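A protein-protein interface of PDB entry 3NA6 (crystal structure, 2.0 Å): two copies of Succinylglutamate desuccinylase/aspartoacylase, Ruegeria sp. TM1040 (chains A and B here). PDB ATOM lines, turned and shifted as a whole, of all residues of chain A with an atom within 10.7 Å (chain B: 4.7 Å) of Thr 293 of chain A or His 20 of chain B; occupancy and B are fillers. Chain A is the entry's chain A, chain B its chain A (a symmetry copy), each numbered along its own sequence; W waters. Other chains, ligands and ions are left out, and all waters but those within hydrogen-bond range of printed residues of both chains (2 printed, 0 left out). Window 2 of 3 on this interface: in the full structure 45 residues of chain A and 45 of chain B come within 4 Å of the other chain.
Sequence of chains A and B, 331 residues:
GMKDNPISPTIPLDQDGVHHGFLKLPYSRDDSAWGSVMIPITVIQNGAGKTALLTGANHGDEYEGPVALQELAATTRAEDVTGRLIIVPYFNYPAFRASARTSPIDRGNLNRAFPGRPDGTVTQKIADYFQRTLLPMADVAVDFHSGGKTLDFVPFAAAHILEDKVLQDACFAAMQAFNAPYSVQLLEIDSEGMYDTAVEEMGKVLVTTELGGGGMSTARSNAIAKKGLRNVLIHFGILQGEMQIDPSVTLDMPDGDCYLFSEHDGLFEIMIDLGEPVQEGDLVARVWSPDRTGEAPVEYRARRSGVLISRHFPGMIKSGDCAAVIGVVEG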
ATOM      1  N   LEU A 267      20.049   8.941 -32.738  1.00  0.00           N
ATOM      2  CA  LEU A 267      20.472   9.816 -31.658  1.00  0.00           C
ATOM      3  C   LEU A 267      21.994   9.797 -31.583  1.00  0.00           C
ATOM      4  O   LEU A 267      22.604   8.769 -31.331  1.00  0.00           O
ATOM      5  CB  LEU A 267      19.879   9.337 -30.321  1.00  0.00           C
ATOM      6  CG  LEU A 267      20.217  10.130 -29.049  1.00  0.00           C
ATOM      7  CD1 LEU A 267      19.744  11.552 -29.234  1.00  0.00           C
ATOM      8  CD2 LEU A 267      19.621   9.504 -27.762  1.00  0.00           C
ATOM      9  N   TRP A 288      22.512   5.887 -31.395  1.00  0.00           N
ATOM     10  CA  TRP A 288      21.459   5.148 -30.675  1.00  0.00           C
ATOM     11  C   TRP A 288      20.201   5.156 -31.545  1.00  0.00           C
ATOM     12  O   TRP A 288      19.967   6.086 -32.305  1.00  0.00           O
ATOM     13  CB  TRP A 288      21.148   5.786 -29.323  1.00  0.00           C
ATOM     14  CG  TRP A 288      22.261   5.752 -28.339  1.00  0.00           C
ATOM     15  CD1 TRP A 288      23.261   6.681 -28.178  1.00  0.00           C
ATOM     16  CD2 TRP A 288      22.522   4.717 -27.393  1.00  0.00           C
ATOM     17  NE1 TRP A 288      24.112   6.284 -27.160  1.00  0.00           N
ATOM     18  CE2 TRP A 288      23.700   5.069 -26.688  1.00  0.00           C
ATOM     19  CE3 TRP A 288      21.872   3.521 -27.067  1.00  0.00           C
ATOM     20  CZ2 TRP A 288      24.230   4.268 -25.664  1.00  0.00           C
ATOM     21  CZ3 TRP A 288      22.420   2.717 -26.087  1.00  0.00           C
ATOM     22  CH2 TRP A 288      23.577   3.104 -25.386  1.00  0.00           C
ATOM     23  N   SER A 289      19.403   4.120 -31.425  1.00  0.00           N
ATOM     24  CA  SER A 289      18.156   4.004 -32.160  1.00  0.00           C
ATOM     25  C   SER A 289      17.258   5.147 -31.814  1.00  0.00           C
ATOM     26  O   SER A 289      16.992   5.401 -30.620  1.00  0.00           O
ATOM     27  CB  SER A 289      17.413   2.704 -31.807  1.00  0.00           C
ATOM     28  OG  SER A 289      16.126   2.673 -32.414  1.00  0.00           O
ATOM     29  N   PRO A 290      16.732   5.813 -32.848  1.00  0.00           N
ATOM     30  CA  PRO A 290      15.743   6.859 -32.663  1.00  0.00           C
ATOM     31  C   PRO A 290      14.336   6.351 -32.449  1.00  0.00           C
ATOM     32  O   PRO A 290      13.444   7.152 -32.254  1.00  0.00           O
ATOM     33  CB  PRO A 290      15.782   7.584 -34.001  1.00  0.00           C
ATOM     34  CG  PRO A 290      15.898   6.496 -34.958  1.00  0.00           C
ATOM     35  CD  PRO A 290      16.880   5.482 -34.282  1.00  0.00           C
ATOM     36  N   ASP A 291      14.106   5.050 -32.521  1.00  0.00           N
ATOM     37  CA  ASP A 291      12.724   4.599 -32.413  1.00  0.00           C
ATOM     38  C   ASP A 291      12.420   3.384 -31.520  1.00  0.00           C
ATOM     39  O   ASP A 291      11.300   2.900 -31.505  1.00  0.00           O
ATOM     40  CB  ASP A 291      12.148   4.390 -33.796  1.00  0.00           C
ATOM     41  CG  ASP A 291      12.865   3.326 -34.593  1.00  0.00           C
ATOM     42  OD1 ASP A 291      13.587   2.486 -34.044  1.00  0.00           O
ATOM     43  OD2 ASP A 291      12.652   3.316 -35.811  1.00  0.00           O
ATOM     44  N   ARG A 292      13.404   2.916 -30.779  1.00  0.00           N
ATOM     45  CA  ARG A 292      13.165   1.912 -29.758  1.00  0.00           C
ATOM     46  C   ARG A 292      14.242   1.967 -28.666  1.00  0.00           C
ATOM     47  O   ARG A 292      15.273   2.638 -28.804  1.00  0.00           O
ATOM     48  CB  ARG A 292      13.099   0.502 -30.379  1.00  0.00           C
ATOM     49  CG  ARG A 292      14.366   0.011 -31.083  1.00  0.00           C
ATOM     50  CD  ARG A 292      14.014  -1.010 -32.219  1.00  0.00           C
ATOM     51  NE  ARG A 292      13.292  -0.355 -33.316  1.00  0.00           N
ATOM     52  CZ  ARG A 292      12.049  -0.638 -33.739  1.00  0.00           C
ATOM     53  NH1 ARG A 292      11.326  -1.620 -33.213  1.00  0.00           N
ATOM     54  NH2 ARG A 292      11.520   0.079 -34.730  1.00  0.00           N
ATOM     55  N   THR A 293      13.981   1.262 -27.572  1.00  0.00           N
ATOM     56  CA  THR A 293      14.937   1.105 -26.501  1.00  0.00           C
ATOM     57  C   THR A 293      15.482  -0.308 -26.492  1.00  0.00           C
ATOM     58  O   THR A 293      14.900  -1.233 -27.072  1.00  0.00           O
ATOM     59  CB  THR A 293      14.270   1.345 -25.126  1.00  0.00           C
ATOM     60  OG1 THR A 293      13.152   0.458 -24.994  1.00  0.00           O
ATOM     61  CG2 THR A 293      13.811   2.860 -25.010  1.00  0.00           C
ATOM     62  N   GLY A 294      16.598  -0.462 -25.799  1.00  0.00           N
ATOM     63  CA  GLY A 294      17.158  -1.779 -25.499  1.00  0.00           C
ATOM     64  C   GLY A 294      18.151  -2.273 -26.527  1.00  0.00           C
ATOM     65  O   GLY A 294      18.744  -3.323 -26.340  1.00  0.00           O
ATOM     66  N   GLU A 295      18.356  -1.522 -27.604  1.00  0.00           N
ATOM     67  CA  GLU A 295      19.207  -1.975 -28.695  1.00  0.00           C
ATOM     68  C   GLU A 295      20.645  -1.490 -28.480  1.00  0.00           C
ATOM     69  O   GLU A 295      20.862  -0.357 -28.084  1.00  0.00           O
ATOM     70  CB  GLU A 295      18.644  -1.422 -30.008  1.00  0.00           C
ATOM     71  CG  GLU A 295      19.027  -2.151 -31.272  1.00  0.00           C
ATOM     72  CD  GLU A 295      18.242  -1.648 -32.503  1.00  0.00           C
ATOM     73  OE1 GLU A 295      18.690  -0.690 -33.176  1.00  0.00           O
ATOM     74  OE2 GLU A 295      17.182  -2.224 -32.796  1.00  0.00           O
ATOM     75  N   ALA A 296      21.635  -2.340 -28.754  1.00  0.00           N
ATOM     76  CA  ALA A 296      23.026  -1.904 -28.717  1.00  0.00           C
ATOM     77  C   ALA A 296      23.236  -0.787 -29.741  1.00  0.00           C
ATOM     78  O   ALA A 296      22.739  -0.860 -30.871  1.00  0.00           O
ATOM     79  CB  ALA A 296      23.994  -3.076 -29.001  1.00  0.00           C
ATOM     80  N   PRO A 297      23.967   0.251 -29.357  1.00  0.00           N
ATOM     81  CA  PRO A 297      24.236   1.384 -30.257  1.00  0.00           C
ATOM     82  C   PRO A 297      25.249   1.008 -31.325  1.00  0.00           C
ATOM     83  O   PRO A 297      25.933   0.031 -31.153  1.00  0.00           O
ATOM     84  CB  PRO A 297      24.831   2.426 -29.324  1.00  0.00           C
ATOM     85  CG  PRO A 297      25.459   1.651 -28.201  1.00  0.00           C
ATOM     86  CD  PRO A 297      24.716   0.343 -28.087  1.00  0.00           C
ATOM     87  N   ILE B  11       4.371  -4.154 -23.389  1.00  0.00           N
ATOM     88  CA  ILE B  11       5.065  -4.949 -22.390  1.00  0.00           C
ATOM     89  C   ILE B  11       4.357  -4.762 -21.067  1.00  0.00           C
ATOM     90  O   ILE B  11       3.629  -3.772 -20.880  1.00  0.00           O
ATOM     91  CB  ILE B  11       6.513  -4.511 -22.182  1.00  0.00           C
ATOM     92  CG1 ILE B  11       6.590  -3.006 -21.964  1.00  0.00           C
ATOM     93  CG2 ILE B  11       7.388  -4.968 -23.323  1.00  0.00           C
ATOM     94  CD1 ILE B  11       7.915  -2.533 -21.312  1.00  0.00           C
ATOM     95  N   VAL B  18      13.913  -7.221 -17.267  1.00  0.00           N
ATOM     96  CA  VAL B  18      14.170  -6.118 -18.199  1.00  0.00           C
ATOM     97  C   VAL B  18      13.195  -6.280 -19.373  1.00  0.00           C
ATOM     98  O   VAL B  18      13.142  -7.316 -20.012  1.00  0.00           O
ATOM     99  CB  VAL B  18      15.628  -6.137 -18.658  1.00  0.00           C
ATOM    100  CG1 VAL B  18      15.877  -5.154 -19.839  1.00  0.00           C
ATOM    101  CG2 VAL B  18      16.599  -5.835 -17.456  1.00  0.00           C
ATOM    102  N   HIS B  19      12.377  -5.275 -19.623  1.00  0.00           N
ATOM    103  CA  HIS B  19      11.390  -5.355 -20.693  1.00  0.00           C
ATOM    104  C   HIS B  19      11.483  -4.122 -21.562  1.00  0.00           C
ATOM    105  O   HIS B  19      11.449  -3.023 -21.033  1.00  0.00           O
ATOM    106  CB  HIS B  19      10.007  -5.400 -20.081  1.00  0.00           C
ATOM    107  CG  HIS B  19       9.731  -6.669 -19.345  1.00  0.00           C
ATOM    108  ND1 HIS B  19      10.001  -6.821 -18.002  1.00  0.00           N
ATOM    109  CD2 HIS B  19       9.266  -7.861 -19.781  1.00  0.00           C
ATOM    110  CE1 HIS B  19       9.667  -8.044 -17.635  1.00  0.00           C
ATOM    111  NE2 HIS B  19       9.218  -8.693 -18.698  1.00  0.00           N
ATOM    112  N   HIS B  20      11.558  -4.312 -22.876  1.00  0.00           N
ATOM    113  CA  HIS B  20      11.674  -3.219 -23.833  1.00  0.00           C
ATOM    114  C   HIS B  20      10.495  -3.297 -24.788  1.00  0.00           C
ATOM    115  O   HIS B  20      10.238  -4.338 -25.402  1.00  0.00           O
ATOM    116  CB  HIS B  20      12.957  -3.338 -24.668  1.00  0.00           C
ATOM    117  CG  HIS B  20      14.217  -3.496 -23.864  1.00  0.00           C
ATOM    118  ND1 HIS B  20      14.714  -2.503 -23.039  1.00  0.00           N
ATOM    119  CD2 HIS B  20      15.126  -4.504 -23.828  1.00  0.00           C
ATOM    120  CE1 HIS B  20      15.852  -2.912 -22.507  1.00  0.00           C
ATOM    121  NE2 HIS B  20      16.131  -4.118 -22.973  1.00  0.00           N
ATOM    122  N   GLY B  21       9.783  -2.193 -24.925  1.00  0.00           N
ATOM    123  CA  GLY B  21       8.645  -2.154 -25.813  1.00  0.00           C
ATOM    124  C   GLY B  21       8.176  -0.752 -26.077  1.00  0.00           C
ATOM    125  O   GLY B  21       9.000   0.155 -26.210  1.00  0.00           O
ATOM    126  N   PRO B  40       8.782   4.615 -27.298  1.00  0.00           N
ATOM    127  CA  PRO B  40       9.644   3.594 -26.690  1.00  0.00           C
ATOM    128  C   PRO B  40       9.627   3.671 -25.187  1.00  0.00           C
ATOM    129  O   PRO B  40       9.566   4.759 -24.622  1.00  0.00           O
ATOM    130  CB  PRO B  40      11.027   3.938 -27.229  1.00  0.00           C
ATOM    131  CG  PRO B  40      10.712   4.530 -28.571  1.00  0.00           C
ATOM    132  CD  PRO B  40       9.557   5.442 -28.228  1.00  0.00           C
ATOM    133  N   ILE B  41       9.669   2.505 -24.553  1.00  0.00           N
ATOM    134  CA  ILE B  41       9.683   2.418 -23.111  1.00  0.00           C
ATOM    135  C   ILE B  41      10.457   1.174 -22.694  1.00  0.00           C
ATOM    136  O   ILE B  41      10.390   0.147 -23.358  1.00  0.00           O
ATOM    137  CB  ILE B  41       8.236   2.418 -22.529  1.00  0.00           C
ATOM    138  CG1 ILE B  41       8.253   2.450 -20.980  1.00  0.00           C
ATOM    139  CG2 ILE B  41       7.406   1.248 -23.078  1.00  0.00           C
ATOM    140  CD1 ILE B  41       6.891   2.836 -20.399  1.00  0.00           C
ATOM    141  N   THR B  42      11.223   1.297 -21.613  1.00  0.00           N
ATOM    142  CA  THR B  42      11.874   0.159 -20.986  1.00  0.00           C
ATOM    143  C   THR B  42      11.472   0.144 -19.514  1.00  0.00           C
ATOM    144  O   THR B  42      11.455   1.194 -18.851  1.00  0.00           O
ATOM    145  CB  THR B  42      13.408   0.237 -21.106  1.00  0.00           C
ATOM    146  OG1 THR B  42      13.810  -0.061 -22.446  1.00  0.00           O
ATOM    147  CG2 THR B  42      14.059  -0.769 -20.177  1.00  0.00           C
ATOM    148  N   GLN B  70      18.812   6.332 -22.920  1.00  0.00           N
ATOM    149  CA  GLN B  70      18.988   5.201 -23.825  1.00  0.00           C
ATOM    150  C   GLN B  70      20.082   4.285 -23.273  1.00  0.00           C
ATOM    151  O   GLN B  70      19.924   3.072 -23.283  1.00  0.00           O
ATOM    152  CB  GLN B  70      19.345   5.605 -25.258  1.00  0.00           C
ATOM    153  CG  GLN B  70      18.186   6.065 -26.097  1.00  0.00           C
ATOM    154  CD  GLN B  70      17.282   4.888 -26.549  1.00  0.00           C
ATOM    155  OE1 GLN B  70      16.861   4.046 -25.744  1.00  0.00           O
ATOM    156  NE2 GLN B  70      16.976   4.853 -27.812  1.00  0.00           N
ATOM    157  N   ALA B  73      18.782   2.308 -20.306  1.00  0.00           N
ATOM    158  CA  ALA B  73      17.817   1.249 -20.658  1.00  0.00           C
ATOM    159  C   ALA B  73      18.537   0.047 -21.286  1.00  0.00           C
ATOM    160  O   ALA B  73      18.112  -1.102 -21.125  1.00  0.00           O
ATOM    161  CB  ALA B  73      16.754   1.769 -21.609  1.00  0.00           C
ATOM    162  N   PRO B  89      12.955   7.477 -22.850  1.00  0.00           N
ATOM    163  CA  PRO B  89      13.969   8.457 -23.297  1.00  0.00           C
ATOM    164  C   PRO B  89      13.415   9.560 -24.183  1.00  0.00           C
ATOM    165  O   PRO B  89      13.977  10.649 -24.224  1.00  0.00           O
ATOM    166  CB  PRO B  89      14.981   7.619 -24.079  1.00  0.00           C
ATOM    167  CG  PRO B  89      14.521   6.188 -23.992  1.00  0.00           C
ATOM    168  CD  PRO B  89      13.165   6.133 -23.409  1.00  0.00           C
HETATM  169  O   HOH W   1      18.078   2.034 -24.989  1.00  0.00           O
HETATM  170  O   HOH W   2      11.536  -0.280 -27.072  1.00  0.00           O
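Of the 11 printed residues of chain B, 6 touch a printed residue of chain A.
Among the printed residues, no Asp or Glu carboxylate lies within 4 Å of a Lys or Arg side-chain nitrogen of the other chain.
Of chain B, only His 20, Pro 40, Ile 41, Thr 42, Gln 70 and Pro 89 come within 4 Å of Thr 293 of chain A.
His 20 of chain B touches two residues of chain A.
No residue of chain A comes within 4 Å of Gly 21 of chain B.
Thr 42 of chain B touches just one residue of chain A: Thr 293 (2.7 Å).
No residue of chain A comes within 4 Å of Ala 73 of chain B.
Printed residues of chain B within 4 Å of Trp 288 of chain A: Gln 70 (3.7 Å).
Printed residues of chain B within 4 Å of Ser 289 of chain A: Gln 70.
Glu 295 of chain A touches none of the printed residues of chain B.
Ile 11 of chain B touches none of the printed residues of chain A.
The nearest residue of chain B that does not touch Thr 293 of chain A is Gly 21 of chain B (4.3 Å).
The nearest residue of chain A that does not touch His 20 of chain B is Glu 295 of chain A (5.8 Å).
Among the printed residues, pairs that only touch across the chains: Thr 293 of chain A with Gln 70 of chain B (3.4 Å), Asp 291 of chain A with Pro 40 of chain B (3.4 Å), Gly 294 of chain A with His 20 of chain B (3.5 Å), Thr 293 of chain A with Pro 89 of chain B (3.6 Å), Thr 293 of chain A with Pro 40 of chain B (3.7 Å), Thr 293 of chain A with His 20 of chain B (3.7 Å), Trp 288 of chain A with Gln 70 of chain B (3.7 Å) and Arg 292 of chain A with Pro 40 of chain B (3.8 Å).
No position is printed for both chains.
The side-chain amide nitrogen of Gln 70 of chain B lies within hydrogen-bond range of the backbone carbonyl oxygen of Ser 289 of chain A, at 2.9 Å.
The side-chain amide nitrogen (NE2) of Gln 70 of chain B sits at hydrogen-bond distance from the backbone carbonyl oxygen (O) of Arg 292 of chain A (3.0 Å).
OG1 of Thr 293 of chain A sits at hydrogen-bond distance from O of Ile 41 of chain B (3.2 Å).
OG1 of Thr 293 of chain A lies within hydrogen-bond range of OG1 of Thr 42 of chain B, 2.7 Å away.
The backbone NH (N) of Trp 288 of chain A is in hydrogen-bond range of the backbone carbonyl oxygen (O) of Leu 267 of chain A (2.9 Å).
OD1 of Asp 291 of chain A lies within hydrogen-bond range of OG of Ser 289 of chain A.
OG of Ser 289 of chain A lies within hydrogen-bond range of N of Arg 292 of chain A.
The guanidinium group (NE) of Arg 292 of chain A lies within salt-bridge range of the side-chain carboxylate (OD1) of Asp 291 of chain A (2.9 Å).
A ring nitrogen (ND1) of His 20 of chain B sits at hydrogen-bond distance from the side-chain hydroxyl of Thr 42 of chain B.
N of Gly 21 of chain B is in hydrogen-bond range of O of Ile 41 of chain B (2.9 Å).
Water W1 bridges OE1 of Gln 70 of chain B (2.5 Å) and N of Gly 294 of chain A (3.0 Å).
Water W2 lies within hydrogen-bond range of O of Gly 21 of chain B (2.7 Å) and OG1 of Thr 293 of chain A (2.7 Å).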
